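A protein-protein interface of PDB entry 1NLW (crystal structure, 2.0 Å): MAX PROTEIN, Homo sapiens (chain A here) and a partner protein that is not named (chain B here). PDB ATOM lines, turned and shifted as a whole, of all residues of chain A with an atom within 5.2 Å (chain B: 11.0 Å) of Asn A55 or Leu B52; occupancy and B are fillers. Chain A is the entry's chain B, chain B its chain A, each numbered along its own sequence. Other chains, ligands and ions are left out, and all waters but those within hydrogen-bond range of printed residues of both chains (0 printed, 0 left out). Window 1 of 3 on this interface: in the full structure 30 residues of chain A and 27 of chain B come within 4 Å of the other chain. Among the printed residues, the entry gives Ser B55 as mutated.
The side-chain hydroxyl of Tyr A50 sits at hydrogen-bond distance from the side-chain amino group of Lys A54 (2.8 Å). O of Lys B51 is in hydrogen-bond range of OG of Ser B55. SD of Met A51 is in hydrogen-bond range of NZ of Lys A54 (3.6 Å). ND1 of His A58 lies close to O of Lys A54 (3.5 Å). O of Met A51 sits close to OD1 of Asn A55, at 3.5 Å.
O of Leu B52 sits close to OD1 of Asn A55. The backbone NH of Val B27 lies close to the guanidinium group of Arg A52 (2.8 Å). A ring nitrogen (NE2) of His B48 lies within hydrogen-bond range of the guanidinium group (NH2) of Arg A52.
Ile A48 touches Leu B23. Val B27 touches Ile A48 (CG2 to CD1, 3.8 Å). CG1 of Ile A48 touches CG1 of Ile B49 (3.5 Å). Leu B52 touches Ile A48. Met A51 touches Asp B56 (CE to CB, 3.8 Å). NH1 of Arg A52 touches CD2 of Leu B26 (3.5 Å). Arg A52 touches Leu B52 (CG to CD2, 3.98 Å). CA of Asp B56 touches ND2 of Asn A55, 3.3 Å away. His A58 touches Asp B56. Ala B59 touches His A58 (CB to CB, 3.9 Å).
Asn A55 touches just these residues of chain B: Leu B52 (2.9 Å), Ser B55 (3.9 Å) and Asp B56 (3.3 Å). Of the printed residues of chain A, Leu B52 touches Ile A48 (3.9 Å), Met A51 (3.8 Å), Arg A52 (3.98 Å) and Asn A55 (2.9 Å). Met A51 touches two residues of chain B. Arg A52 touches four residues of chain B. Lys A54 touches just one residue of chain B: Asp B56. No residue of chain B comes within 4 Å of His A56. No residue of chain B comes within 4 Å of Thr A57. No residue of chain B comes within 4 Å of Gln A59. Of the printed residues of chain A, Leu B23 touches Ile A48. Of the printed residues of chain B, His A58 touches Asp B56, Ala B59 and Ile B63. Of the printed residues of chain A, His B48 touches Arg A52. Printed residues of chain A within 4 Å of Ala B59: His A58 (3.9 Å). Of the printed residues of chain A, Leu B26 touches Arg A52. Glu B53 touches none of the printed residues of chain A. His B61 touches none of the printed residues of chain A. The nearest printed residue of chain A that does not touch Leu B52 is Tyr A50 (6.7 Å).
Of the 11 printed residues of chain A, 6 touch a printed residue of chain B. Printed residues of chain A that touch a printed residue of chain B: Ile A48, Met A51, Arg A52, Lys A54, Asn A55 and His A58. Hydrophobic or aromatic side chains of chain A within 4 Å of the printed part of chain B: Ile A48, Met A51 and His A58. Among the printed residues, 17 pairs touch across the chains. Among the printed residues, no Asp or Glu carboxylate lies within 4 Å of a Lys or Arg side-chain nitrogen of the other chain.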
ATOM      1  N   ILE A  48     -14.617 -11.434 -20.434  1.00  0.00           N
ATOM      2  CA  ILE A  48     -15.031 -10.418 -19.454  1.00  0.00           C
ATOM      3  C   ILE A  48     -13.820  -9.619 -18.964  1.00  0.00           C
ATOM      4  O   ILE A  48     -13.897  -8.395 -18.806  1.00  0.00           O
ATOM      5  CB  ILE A  48     -15.727 -11.052 -18.195  1.00  0.00           C
ATOM      6  CG1 ILE A  48     -17.198 -11.363 -18.488  1.00  0.00           C
ATOM      7  CG2 ILE A  48     -15.634 -10.101 -17.003  1.00  0.00           C
ATOM      8  CD1 ILE A  48     -17.848 -12.257 -17.437  1.00  0.00           C
ATOM      9  N   TYR A  50     -11.025  -9.250 -20.577  1.00  0.00           N
ATOM     10  CA  TYR A  50     -10.603  -8.506 -21.753  1.00  0.00           C
ATOM     11  C   TYR A  50     -11.449  -7.244 -21.945  1.00  0.00           C
ATOM     12  O   TYR A  50     -10.908  -6.136 -22.088  1.00  0.00           O
ATOM     13  CB  TYR A  50     -10.720  -9.389 -22.995  1.00  0.00           C
ATOM     14  CG  TYR A  50     -10.618  -8.630 -24.301  1.00  0.00           C
ATOM     15  CD1 TYR A  50      -9.415  -8.048 -24.703  1.00  0.00           C
ATOM     16  CD2 TYR A  50     -11.731  -8.488 -25.136  1.00  0.00           C
ATOM     17  CE1 TYR A  50      -9.322  -7.350 -25.906  1.00  0.00           C
ATOM     18  CE2 TYR A  50     -11.649  -7.793 -26.338  1.00  0.00           C
ATOM     19  CZ  TYR A  50     -10.443  -7.229 -26.718  1.00  0.00           C
ATOM     20  OH  TYR A  50     -10.349  -6.559 -27.925  1.00  0.00           O
ATOM     21  N   MET A  51     -12.770  -7.416 -21.957  1.00  0.00           N
ATOM     22  CA  MET A  51     -13.688  -6.293 -22.150  1.00  0.00           C
ATOM     23  C   MET A  51     -13.613  -5.221 -21.076  1.00  0.00           C
ATOM     24  O   MET A  51     -13.820  -4.041 -21.352  1.00  0.00           O
ATOM     25  CB  MET A  51     -15.129  -6.807 -22.268  1.00  0.00           C
ATOM     26  CG  MET A  51     -15.381  -7.601 -23.542  1.00  0.00           C
ATOM     27  SD  MET A  51     -15.040  -6.626 -25.026  1.00  0.00           S
ATOM     28  CE  MET A  51     -16.114  -5.275 -24.762  1.00  0.00           C
ATOM     29  N   ARG A  52     -13.343  -5.619 -19.837  1.00  0.00           N
ATOM     30  CA  ARG A  52     -13.228  -4.639 -18.766  1.00  0.00           C
ATOM     31  C   ARG A  52     -11.975  -3.796 -19.011  1.00  0.00           C
ATOM     32  O   ARG A  52     -11.993  -2.586 -18.828  1.00  0.00           O
ATOM     33  CB  ARG A  52     -13.140  -5.337 -17.402  1.00  0.00           C
ATOM     34  CG  ARG A  52     -14.499  -5.794 -16.874  1.00  0.00           C
ATOM     35  CD  ARG A  52     -14.393  -6.511 -15.534  1.00  0.00           C
ATOM     36  NE  ARG A  52     -15.697  -6.978 -15.065  1.00  0.00           N
ATOM     37  CZ  ARG A  52     -15.881  -7.696 -13.960  1.00  0.00           C
ATOM     38  NH1 ARG A  52     -14.842  -8.032 -13.202  1.00  0.00           N
ATOM     39  NH2 ARG A  52     -17.105  -8.076 -13.608  1.00  0.00           N
ATOM     40  N   ARG A  53     -10.894  -4.447 -19.423  1.00  0.00           N
ATOM     41  CA  ARG A  53      -9.642  -3.748 -19.718  1.00  0.00           C
ATOM     42  C   ARG A  53      -9.826  -2.772 -20.878  1.00  0.00           C
ATOM     43  O   ARG A  53      -9.388  -1.634 -20.808  1.00  0.00           O
ATOM     44  CB  ARG A  53      -8.537  -4.742 -20.070  1.00  0.00           C
ATOM     45  CG  ARG A  53      -8.008  -5.545 -18.885  1.00  0.00           C
ATOM     46  CD  ARG A  53      -6.743  -6.311 -19.265  1.00  0.00           C
ATOM     47  NE  ARG A  53      -5.812  -5.453 -19.997  1.00  0.00           N
ATOM     48  CZ  ARG A  53      -4.538  -5.750 -20.245  1.00  0.00           C
ATOM     49  NH1 ARG A  53      -4.022  -6.900 -19.817  1.00  0.00           N
ATOM     50  NH2 ARG A  53      -3.781  -4.897 -20.927  1.00  0.00           N
ATOM     51  N   LYS A  54     -10.481  -3.228 -21.940  1.00  0.00           N
ATOM     52  CA  LYS A  54     -10.734  -2.391 -23.120  1.00  0.00           C
ATOM     53  C   LYS A  54     -11.591  -1.160 -22.778  1.00  0.00           C
ATOM     54  O   LYS A  54     -11.279  -0.040 -23.184  1.00  0.00           O
ATOM     55  CB  LYS A  54     -11.427  -3.223 -24.211  1.00  0.00           C
ATOM     56  CG  LYS A  54     -11.880  -2.410 -25.434  1.00  0.00           C
ATOM     57  CD  LYS A  54     -12.759  -3.246 -26.364  1.00  0.00           C
ATOM     58  CE  LYS A  54     -11.975  -4.354 -27.005  1.00  0.00           C
ATOM     59  NZ  LYS A  54     -12.883  -5.389 -27.571  1.00  0.00           N
ATOM     60  N   ASN A  55     -12.666  -1.372 -22.030  1.00  0.00           N
ATOM     61  CA  ASN A  55     -13.560  -0.285 -21.643  1.00  0.00           C
ATOM     62  C   ASN A  55     -12.878   0.737 -20.734  1.00  0.00           C
ATOM     63  O   ASN A  55     -13.215   1.915 -20.761  1.00  0.00           O
ATOM     64  CB  ASN A  55     -14.817  -0.849 -20.970  1.00  0.00           C
ATOM     65  CG  ASN A  55     -15.772  -1.508 -21.971  1.00  0.00           C
ATOM     66  OD1 ASN A  55     -16.744  -2.157 -21.586  1.00  0.00           O
ATOM     67  ND2 ASN A  55     -15.493  -1.338 -23.262  1.00  0.00           N
ATOM     68  N   HIS A  56     -11.920   0.289 -19.927  1.00  0.00           N
ATOM     69  CA  HIS A  56     -11.196   1.203 -19.055  1.00  0.00           C
ATOM     70  C   HIS A  56     -10.251   2.064 -19.900  1.00  0.00           C
ATOM     71  O   HIS A  56     -10.196   3.283 -19.739  1.00  0.00           O
ATOM     72  CB  HIS A  56     -10.398   0.424 -18.008  1.00  0.00           C
ATOM     73  CG  HIS A  56      -9.388   1.258 -17.290  1.00  0.00           C
ATOM     74  ND1 HIS A  56      -9.732   2.374 -16.557  1.00  0.00           N
ATOM     75  CD2 HIS A  56      -8.036   1.193 -17.265  1.00  0.00           C
ATOM     76  CE1 HIS A  56      -8.633   2.966 -16.121  1.00  0.00           C
ATOM     77  NE2 HIS A  56      -7.591   2.268 -16.536  1.00  0.00           N
ATOM     78  N   THR A  57      -9.512   1.416 -20.797  1.00  0.00           N
ATOM     79  CA  THR A  57      -8.583   2.107 -21.679  1.00  0.00           C
ATOM     80  C   THR A  57      -9.315   3.185 -22.482  1.00  0.00           C
ATOM     81  O   THR A  57      -8.809   4.297 -22.629  1.00  0.00           O
ATOM     82  CB  THR A  57      -7.918   1.116 -22.652  1.00  0.00           C
ATOM     83  OG1 THR A  57      -7.046   0.247 -21.921  1.00  0.00           O
ATOM     84  CG2 THR A  57      -7.126   1.854 -23.722  1.00  0.00           C
ATOM     85  N   HIS A  58     -10.496   2.851 -23.008  1.00  0.00           N
ATOM     86  CA  HIS A  58     -11.283   3.814 -23.775  1.00  0.00           C
ATOM     87  C   HIS A  58     -11.799   4.933 -22.888  1.00  0.00           C
ATOM     88  O   HIS A  58     -11.923   6.076 -23.330  1.00  0.00           O
ATOM     89  CB  HIS A  58     -12.462   3.131 -24.461  1.00  0.00           C
ATOM     90  CG  HIS A  58     -12.063   2.273 -25.617  1.00  0.00           C
ATOM     91  ND1 HIS A  58     -12.805   1.187 -26.025  1.00  0.00           N
ATOM     92  CD2 HIS A  58     -10.972   2.308 -26.418  1.00  0.00           C
ATOM     93  CE1 HIS A  58     -12.182   0.584 -27.022  1.00  0.00           C
ATOM     94  NE2 HIS A  58     -11.067   1.245 -27.280  1.00  0.00           N
ATOM     95  N   GLN A  59     -12.109   4.613 -21.635  1.00  0.00           N
ATOM     96  CA  GLN A  59     -12.594   5.639 -20.719  1.00  0.00           C
ATOM     97  C   GLN A  59     -11.513   6.706 -20.577  1.00  0.00           C
ATOM     98  O   GLN A  59     -11.798   7.905 -20.606  1.00  0.00           O
ATOM     99  CB  GLN A  59     -12.922   5.039 -19.353  1.00  0.00           C
ATOM    100  CG  GLN A  59     -13.557   6.037 -18.413  1.00  0.00           C
ATOM    101  CD  GLN A  59     -14.696   6.789 -19.079  1.00  0.00           C
ATOM    102  OE1 GLN A  59     -15.672   6.185 -19.531  1.00  0.00           O
ATOM    103  NE2 GLN A  59     -14.571   8.116 -19.150  1.00  0.00           N
ATOM    104  N   LEU B  23     -15.498 -17.527 -12.320  1.00  0.00           N
ATOM    105  CA  LEU B  23     -16.443 -16.638 -13.005  1.00  0.00           C
ATOM    106  C   LEU B  23     -17.302 -15.927 -11.955  1.00  0.00           C
ATOM    107  O   LEU B  23     -17.678 -14.766 -12.113  1.00  0.00           O
ATOM    108  CB  LEU B  23     -17.337 -17.450 -13.957  1.00  0.00           C
ATOM    109  CG  LEU B  23     -18.357 -16.681 -14.806  1.00  0.00           C
ATOM    110  CD1 LEU B  23     -17.667 -15.534 -15.560  1.00  0.00           C
ATOM    111  CD2 LEU B  23     -19.020 -17.640 -15.795  1.00  0.00           C
ATOM    112  N   LEU B  26     -15.567 -12.794 -10.638  1.00  0.00           N
ATOM    113  CA  LEU B  26     -15.775 -11.616 -11.474  1.00  0.00           C
ATOM    114  C   LEU B  26     -17.285 -11.443 -11.482  1.00  0.00           C
ATOM    115  O   LEU B  26     -17.999 -12.264 -10.909  1.00  0.00           O
ATOM    116  CB  LEU B  26     -15.281 -11.869 -12.901  1.00  0.00           C
ATOM    117  CG  LEU B  26     -13.792 -12.166 -13.058  1.00  0.00           C
ATOM    118  CD1 LEU B  26     -13.482 -12.563 -14.492  1.00  0.00           C
ATOM    119  CD2 LEU B  26     -12.997 -10.941 -12.649  1.00  0.00           C
ATOM    120  N   VAL B  27     -17.781 -10.392 -12.120  1.00  0.00           N
ATOM    121  CA  VAL B  27     -19.223 -10.179 -12.174  1.00  0.00           C
ATOM    122  C   VAL B  27     -19.740  -9.768 -10.803  1.00  0.00           C
ATOM    123  O   VAL B  27     -19.568 -10.495  -9.821  1.00  0.00           O
ATOM    124  CB  VAL B  27     -19.962 -11.474 -12.614  1.00  0.00           C
ATOM    125  CG1 VAL B  27     -21.455 -11.242 -12.638  1.00  0.00           C
ATOM    126  CG2 VAL B  27     -19.469 -11.922 -13.985  1.00  0.00           C
ATOM    127  N   PRO B  28     -20.389  -8.595 -10.715  1.00  0.00           N
ATOM    128  CA  PRO B  28     -20.918  -8.133  -9.428  1.00  0.00           C
ATOM    129  C   PRO B  28     -21.753  -9.207  -8.738  1.00  0.00           C
ATOM    130  O   PRO B  28     -21.844  -9.240  -7.511  1.00  0.00           O
ATOM    131  CB  PRO B  28     -21.738  -6.897  -9.809  1.00  0.00           C
ATOM    132  CG  PRO B  28     -22.122  -7.160 -11.236  1.00  0.00           C
ATOM    133  CD  PRO B  28     -20.851  -7.726 -11.810  1.00  0.00           C
ATOM    134  N   LYS B  44     -26.348 -14.004 -14.859  1.00  0.00           N
ATOM    135  CA  LYS B  44     -25.693 -12.753 -14.559  1.00  0.00           C
ATOM    136  C   LYS B  44     -24.471 -12.518 -15.433  1.00  0.00           C
ATOM    137  O   LYS B  44     -24.224 -11.392 -15.856  1.00  0.00           O
ATOM    138  CB  LYS B  44     -25.273 -12.717 -13.088  1.00  0.00           C
ATOM    139  CG  LYS B  44     -24.785 -11.357 -12.617  1.00  0.00           C
ATOM    140  CD  LYS B  44     -25.941 -10.459 -12.203  1.00  0.00           C
ATOM    141  CE  LYS B  44     -25.486  -9.033 -11.886  1.00  0.00           C
ATOM    142  NZ  LYS B  44     -24.495  -8.937 -10.771  1.00  0.00           N
ATOM    143  N   ALA B  45     -23.700 -13.572 -15.688  1.00  0.00           N
ATOM    144  CA  ALA B  45     -22.510 -13.437 -16.511  1.00  0.00           C
ATOM    145  C   ALA B  45     -22.913 -12.982 -17.924  1.00  0.00           C
ATOM    146  O   ALA B  45     -22.344 -12.036 -18.465  1.00  0.00           O
ATOM    147  CB  ALA B  45     -21.766 -14.759 -16.564  1.00  0.00           C
ATOM    148  N   LYS B  46     -23.904 -13.645 -18.510  1.00  0.00           N
ATOM    149  CA  LYS B  46     -24.350 -13.263 -19.846  1.00  0.00           C
ATOM    150  C   LYS B  46     -24.745 -11.792 -19.885  1.00  0.00           C
ATOM    151  O   LYS B  46     -24.273 -11.034 -20.734  1.00  0.00           O
ATOM    152  CB  LYS B  46     -25.539 -14.114 -20.303  1.00  0.00           C
ATOM    153  CG  LYS B  46     -26.037 -13.712 -21.718  1.00  0.00           C
ATOM    154  CD  LYS B  46     -27.267 -14.489 -22.158  1.00  0.00           C
ATOM    155  CE  LYS B  46     -28.524 -13.958 -21.471  1.00  0.00           C
ATOM    156  NZ  LYS B  46     -29.672 -14.871 -21.763  1.00  0.00           N
ATOM    157  N   LEU B  47     -25.592 -11.374 -18.950  1.00  0.00           N
ATOM    158  CA  LEU B  47     -26.045  -9.987 -18.920  1.00  0.00           C
ATOM    159  C   LEU B  47     -24.917  -8.984 -18.694  1.00  0.00           C
ATOM    160  O   LEU B  47     -24.922  -7.901 -19.286  1.00  0.00           O
ATOM    161  CB  LEU B  47     -27.149  -9.835 -17.877  1.00  0.00           C
ATOM    162  CG  LEU B  47     -28.403 -10.669 -18.203  1.00  0.00           C
ATOM    163  CD1 LEU B  47     -29.440 -10.519 -17.065  1.00  0.00           C
ATOM    164  CD2 LEU B  47     -29.005 -10.223 -19.541  1.00  0.00           C
ATOM    165  N   HIS B  48     -23.935  -9.354 -17.869  1.00  0.00           N
ATOM    166  CA  HIS B  48     -22.780  -8.493 -17.616  1.00  0.00           C
ATOM    167  C   HIS B  48     -21.965  -8.342 -18.923  1.00  0.00           C
ATOM    168  O   HIS B  48     -21.554  -7.232 -19.283  1.00  0.00           O
ATOM    169  CB  HIS B  48     -21.897  -9.093 -16.506  1.00  0.00           C
ATOM    170  CG  HIS B  48     -20.689  -8.267 -16.178  1.00  0.00           C
ATOM    171  ND1 HIS B  48     -20.774  -7.003 -15.637  1.00  0.00           N
ATOM    172  CD2 HIS B  48     -19.368  -8.529 -16.310  1.00  0.00           C
ATOM    173  CE1 HIS B  48     -19.559  -6.518 -15.456  1.00  0.00           C
ATOM    174  NE2 HIS B  48     -18.686  -7.424 -15.856  1.00  0.00           N
ATOM    175  N   ILE B  49     -21.739  -9.445 -19.635  1.00  0.00           N
ATOM    176  CA  ILE B  49     -20.986  -9.380 -20.892  1.00  0.00           C
ATOM    177  C   ILE B  49     -21.726  -8.417 -21.813  1.00  0.00           C
ATOM    178  O   ILE B  49     -21.109  -7.547 -22.422  1.00  0.00           O
ATOM    179  CB  ILE B  49     -20.844 -10.780 -21.564  1.00  0.00           C
ATOM    180  CG1 ILE B  49     -19.809 -11.617 -20.812  1.00  0.00           C
ATOM    181  CG2 ILE B  49     -20.407 -10.639 -23.038  1.00  0.00           C
ATOM    182  CD1 ILE B  49     -19.740 -13.071 -21.260  1.00  0.00           C
ATOM    183  N   LYS B  50     -23.052  -8.567 -21.885  1.00  0.00           N
ATOM    184  CA  LYS B  50     -23.897  -7.706 -22.702  1.00  0.00           C
ATOM    185  C   LYS B  50     -23.687  -6.232 -22.369  1.00  0.00           C
ATOM    186  O   LYS B  50     -23.608  -5.391 -23.265  1.00  0.00           O
ATOM    187  CB  LYS B  50     -25.374  -8.085 -22.503  1.00  0.00           C
ATOM    188  CG  LYS B  50     -26.013  -8.837 -23.669  1.00  0.00           C
ATOM    189  CD  LYS B  50     -25.161  -9.980 -24.198  1.00  0.00           C
ATOM    190  CE  LYS B  50     -25.816 -10.599 -25.426  1.00  0.00           C
ATOM    191  NZ  LYS B  50     -24.952 -11.574 -26.146  1.00  0.00           N
ATOM    192  N   LYS B  51     -23.601  -5.922 -21.078  1.00  0.00           N
ATOM    193  CA  LYS B  51     -23.390  -4.559 -20.619  1.00  0.00           C
ATOM    194  C   LYS B  51     -22.006  -4.055 -21.046  1.00  0.00           C
ATOM    195  O   LYS B  51     -21.864  -2.902 -21.477  1.00  0.00           O
ATOM    196  CB  LYS B  51     -23.519  -4.486 -19.086  1.00  0.00           C
ATOM    197  CG  LYS B  51     -23.296  -3.091 -18.500  1.00  0.00           C
ATOM    198  CD  LYS B  51     -24.338  -2.102 -19.015  1.00  0.00           C
ATOM    199  CE  LYS B  51     -24.120  -0.693 -18.470  1.00  0.00           C
ATOM    200  NZ  LYS B  51     -25.116   0.282 -19.037  1.00  0.00           N
ATOM    201  N   LEU B  52     -20.992  -4.915 -20.928  1.00  0.00           N
ATOM    202  CA  LEU B  52     -19.628  -4.548 -21.319  1.00  0.00           C
ATOM    203  C   LEU B  52     -19.569  -4.192 -22.809  1.00  0.00           C
ATOM    204  O   LEU B  52     -18.886  -3.245 -23.185  1.00  0.00           O
ATOM    205  CB  LEU B  52     -18.640  -5.698 -21.025  1.00  0.00           C
ATOM    206  CG  LEU B  52     -18.426  -5.981 -19.526  1.00  0.00           C
ATOM    207  CD1 LEU B  52     -17.584  -7.228 -19.339  1.00  0.00           C
ATOM    208  CD2 LEU B  52     -17.784  -4.793 -18.883  1.00  0.00           C
ATOM    209  N   GLU B  53     -20.271  -4.963 -23.643  1.00  0.00           N
ATOM    210  CA  GLU B  53     -20.281  -4.711 -25.082  1.00  0.00           C
ATOM    211  C   GLU B  53     -21.029  -3.421 -25.411  1.00  0.00           C
ATOM    212  O   GLU B  53     -20.583  -2.642 -26.246  1.00  0.00           O
ATOM    213  CB  GLU B  53     -20.877  -5.904 -25.844  1.00  0.00           C
ATOM    214  CG  GLU B  53     -19.928  -7.102 -25.913  1.00  0.00           C
ATOM    215  CD  GLU B  53     -20.595  -8.396 -26.363  1.00  0.00           C
ATOM    216  OE1 GLU B  53     -21.834  -8.490 -26.258  1.00  0.00           O
ATOM    217  OE2 GLU B  53     -19.882  -9.335 -26.799  1.00  0.00           O
ATOM    218  N   ASP B  54     -22.144  -3.171 -24.737  1.00  0.00           N
ATOM    219  CA  ASP B  54     -22.891  -1.945 -24.986  1.00  0.00           C
ATOM    220  C   ASP B  54     -22.059  -0.714 -24.594  1.00  0.00           C
ATOM    221  O   ASP B  54     -22.095   0.309 -25.277  1.00  0.00           O
ATOM    222  CB  ASP B  54     -24.216  -1.965 -24.222  1.00  0.00           C
ATOM    223  CG  ASP B  54     -25.083  -0.757 -24.531  1.00  0.00           C
ATOM    224  OD1 ASP B  54     -25.162   0.158 -23.684  1.00  0.00           O
ATOM    225  OD2 ASP B  54     -25.681  -0.728 -25.631  1.00  0.00           O
ATOM    226  N   SER B  55     -21.305  -0.811 -23.503  1.00  0.00           N
ATOM    227  CA  SER B  55     -20.468   0.301 -23.073  1.00  0.00           C
ATOM    228  C   SER B  55     -19.303   0.506 -24.052  1.00  0.00           C
ATOM    229  O   SER B  55     -18.901   1.633 -24.303  1.00  0.00           O
ATOM    230  CB  SER B  55     -19.952   0.069 -21.649  1.00  0.00           C
ATOM    231  OG  SER B  55     -21.013   0.262 -20.728  1.00  0.00           O
ATOM    232  N   ASP B  56     -18.783  -0.588 -24.602  1.00  0.00           N
ATOM    233  CA  ASP B  56     -17.697  -0.526 -25.585  1.00  0.00           C
ATOM    234  C   ASP B  56     -18.220   0.267 -26.791  1.00  0.00           C
ATOM    235  O   ASP B  56     -17.623   1.264 -27.193  1.00  0.00           O
ATOM    236  CB  ASP B  56     -17.302  -1.948 -26.025  1.00  0.00           C
ATOM    237  CG  ASP B  56     -16.374  -1.975 -27.257  1.00  0.00           C
ATOM    238  OD1 ASP B  56     -16.553  -2.873 -28.112  1.00  0.00           O
ATOM    239  OD2 ASP B  56     -15.464  -1.123 -27.369  1.00  0.00           O
ATOM    240  N   ARG B  57     -19.344  -0.177 -27.352  1.00  0.00           N
ATOM    241  CA  ARG B  57     -19.942   0.493 -28.510  1.00  0.00           C
ATOM    242  C   ARG B  57     -20.148   1.984 -28.284  1.00  0.00           C
ATOM    243  O   ARG B  57     -19.871   2.797 -29.168  1.00  0.00           O
ATOM    244  CB  ARG B  57     -21.284  -0.144 -28.876  1.00  0.00           C
ATOM    245  CG  ARG B  57     -21.174  -1.557 -29.409  1.00  0.00           C
ATOM    246  CD  ARG B  57     -22.521  -2.022 -29.963  1.00  0.00           C
ATOM    247  NE  ARG B  57     -23.569  -2.010 -28.947  1.00  0.00           N
ATOM    248  CZ  ARG B  57     -23.837  -3.030 -28.136  1.00  0.00           C
ATOM    249  NH1 ARG B  57     -23.133  -4.152 -28.221  1.00  0.00           N
ATOM    250  NH2 ARG B  57     -24.810  -2.931 -27.235  1.00  0.00           N
ATOM    251  N   LYS B  58     -20.620   2.349 -27.098  1.00  0.00           N
ATOM    252  CA  LYS B  58     -20.853   3.755 -26.794  1.00  0.00           C
ATOM    253  C   LYS B  58     -19.555   4.528 -26.565  1.00  0.00           C
ATOM    254  O   LYS B  58     -19.484   5.731 -26.828  1.00  0.00           O
ATOM    255  CB  LYS B  58     -21.771   3.873 -25.580  1.00  0.00           C
ATOM    256  CG  LYS B  58     -23.146   3.276 -25.843  1.00  0.00           C
ATOM    257  CD  LYS B  58     -24.064   3.408 -24.642  1.00  0.00           C
ATOM    258  CE  LYS B  58     -25.414   2.783 -24.935  1.00  0.00           C
ATOM    259  NZ  LYS B  58     -26.253   2.754 -23.711  1.00  0.00           N
ATOM    260  N   ALA B  59     -18.523   3.842 -26.086  1.00  0.00           N
ATOM    261  CA  ALA B  59     -17.240   4.500 -25.856  1.00  0.00           C
ATOM    262  C   ALA B  59     -16.576   4.780 -27.209  1.00  0.00           C
ATOM    263  O   ALA B  59     -16.112   5.884 -27.455  1.00  0.00           O
ATOM    264  CB  ALA B  59     -16.331   3.621 -24.999  1.00  0.00           C
ATOM    265  N   VAL B  60     -16.535   3.779 -28.080  1.00  0.00           N
ATOM    266  CA  VAL B  60     -15.928   3.962 -29.392  1.00  0.00           C
ATOM    267  C   VAL B  60     -16.618   5.111 -30.133  1.00  0.00           C
ATOM    268  O   VAL B  60     -15.963   5.892 -30.821  1.00  0.00           O
ATOM    269  CB  VAL B  60     -16.017   2.675 -30.241  1.00  0.00           C
ATOM    270  CG1 VAL B  60     -15.511   2.942 -31.662  1.00  0.00           C
ATOM    271  CG2 VAL B  60     -15.183   1.581 -29.594  1.00  0.00           C
ATOM    272  N   HIS B  61     -17.935   5.216 -29.970  1.00  0.00           N
ATOM    273  CA  HIS B  61     -18.718   6.264 -30.618  1.00  0.00           C
ATOM    274  C   HIS B  61     -18.428   7.670 -30.090  1.00  0.00           C
ATOM    275  O   HIS B  61     -18.314   8.626 -30.867  1.00  0.00           O
ATOM    276  CB  HIS B  61     -20.213   5.982 -30.464  1.00  0.00           C
ATOM    277  CG  HIS B  61     -21.080   6.952 -31.204  1.00  0.00           C
ATOM    278  ND1 HIS B  61     -21.182   6.956 -32.580  1.00  0.00           N
ATOM    279  CD2 HIS B  61     -21.849   7.975 -30.765  1.00  0.00           C
ATOM    280  CE1 HIS B  61     -21.979   7.942 -32.956  1.00  0.00           C
ATOM    281  NE2 HIS B  61     -22.395   8.575 -31.874  1.00  0.00           N
ATOM    282  N   GLN B  62     -18.317   7.806 -28.772  1.00  0.00           N
ATOM    283  CA  GLN B  62     -18.044   9.105 -28.174  1.00  0.00           C
ATOM    284  C   GLN B  62     -16.624   9.546 -28.507  1.00  0.00           C
ATOM    285  O   GLN B  62     -16.372  10.735 -28.700  1.00  0.00           O
ATOM    286  CB  GLN B  62     -18.251   9.055 -26.658  1.00  0.00           C
ATOM    287  N   ILE B  63     -15.701   8.591 -28.573  1.00  0.00           N
ATOM    288  CA  ILE B  63     -14.314   8.899 -28.919  1.00  0.00           C
ATOM    289  C   ILE B  63     -14.308   9.517 -30.324  1.00  0.00           C
ATOM    290  O   ILE B  63     -13.683  10.553 -30.558  1.00  0.00           O
ATOM    291  CB  ILE B  63     -13.443   7.616 -28.896  1.00  0.00           C
ATOM    292  CG1 ILE B  63     -13.149   7.223 -27.437  1.00  0.00           C
ATOM    293  CG2 ILE B  63     -12.145   7.822 -29.672  1.00  0.00           C
ATOM    294  CD1 ILE B  63     -12.258   5.983 -27.319  1.00  0.00           C
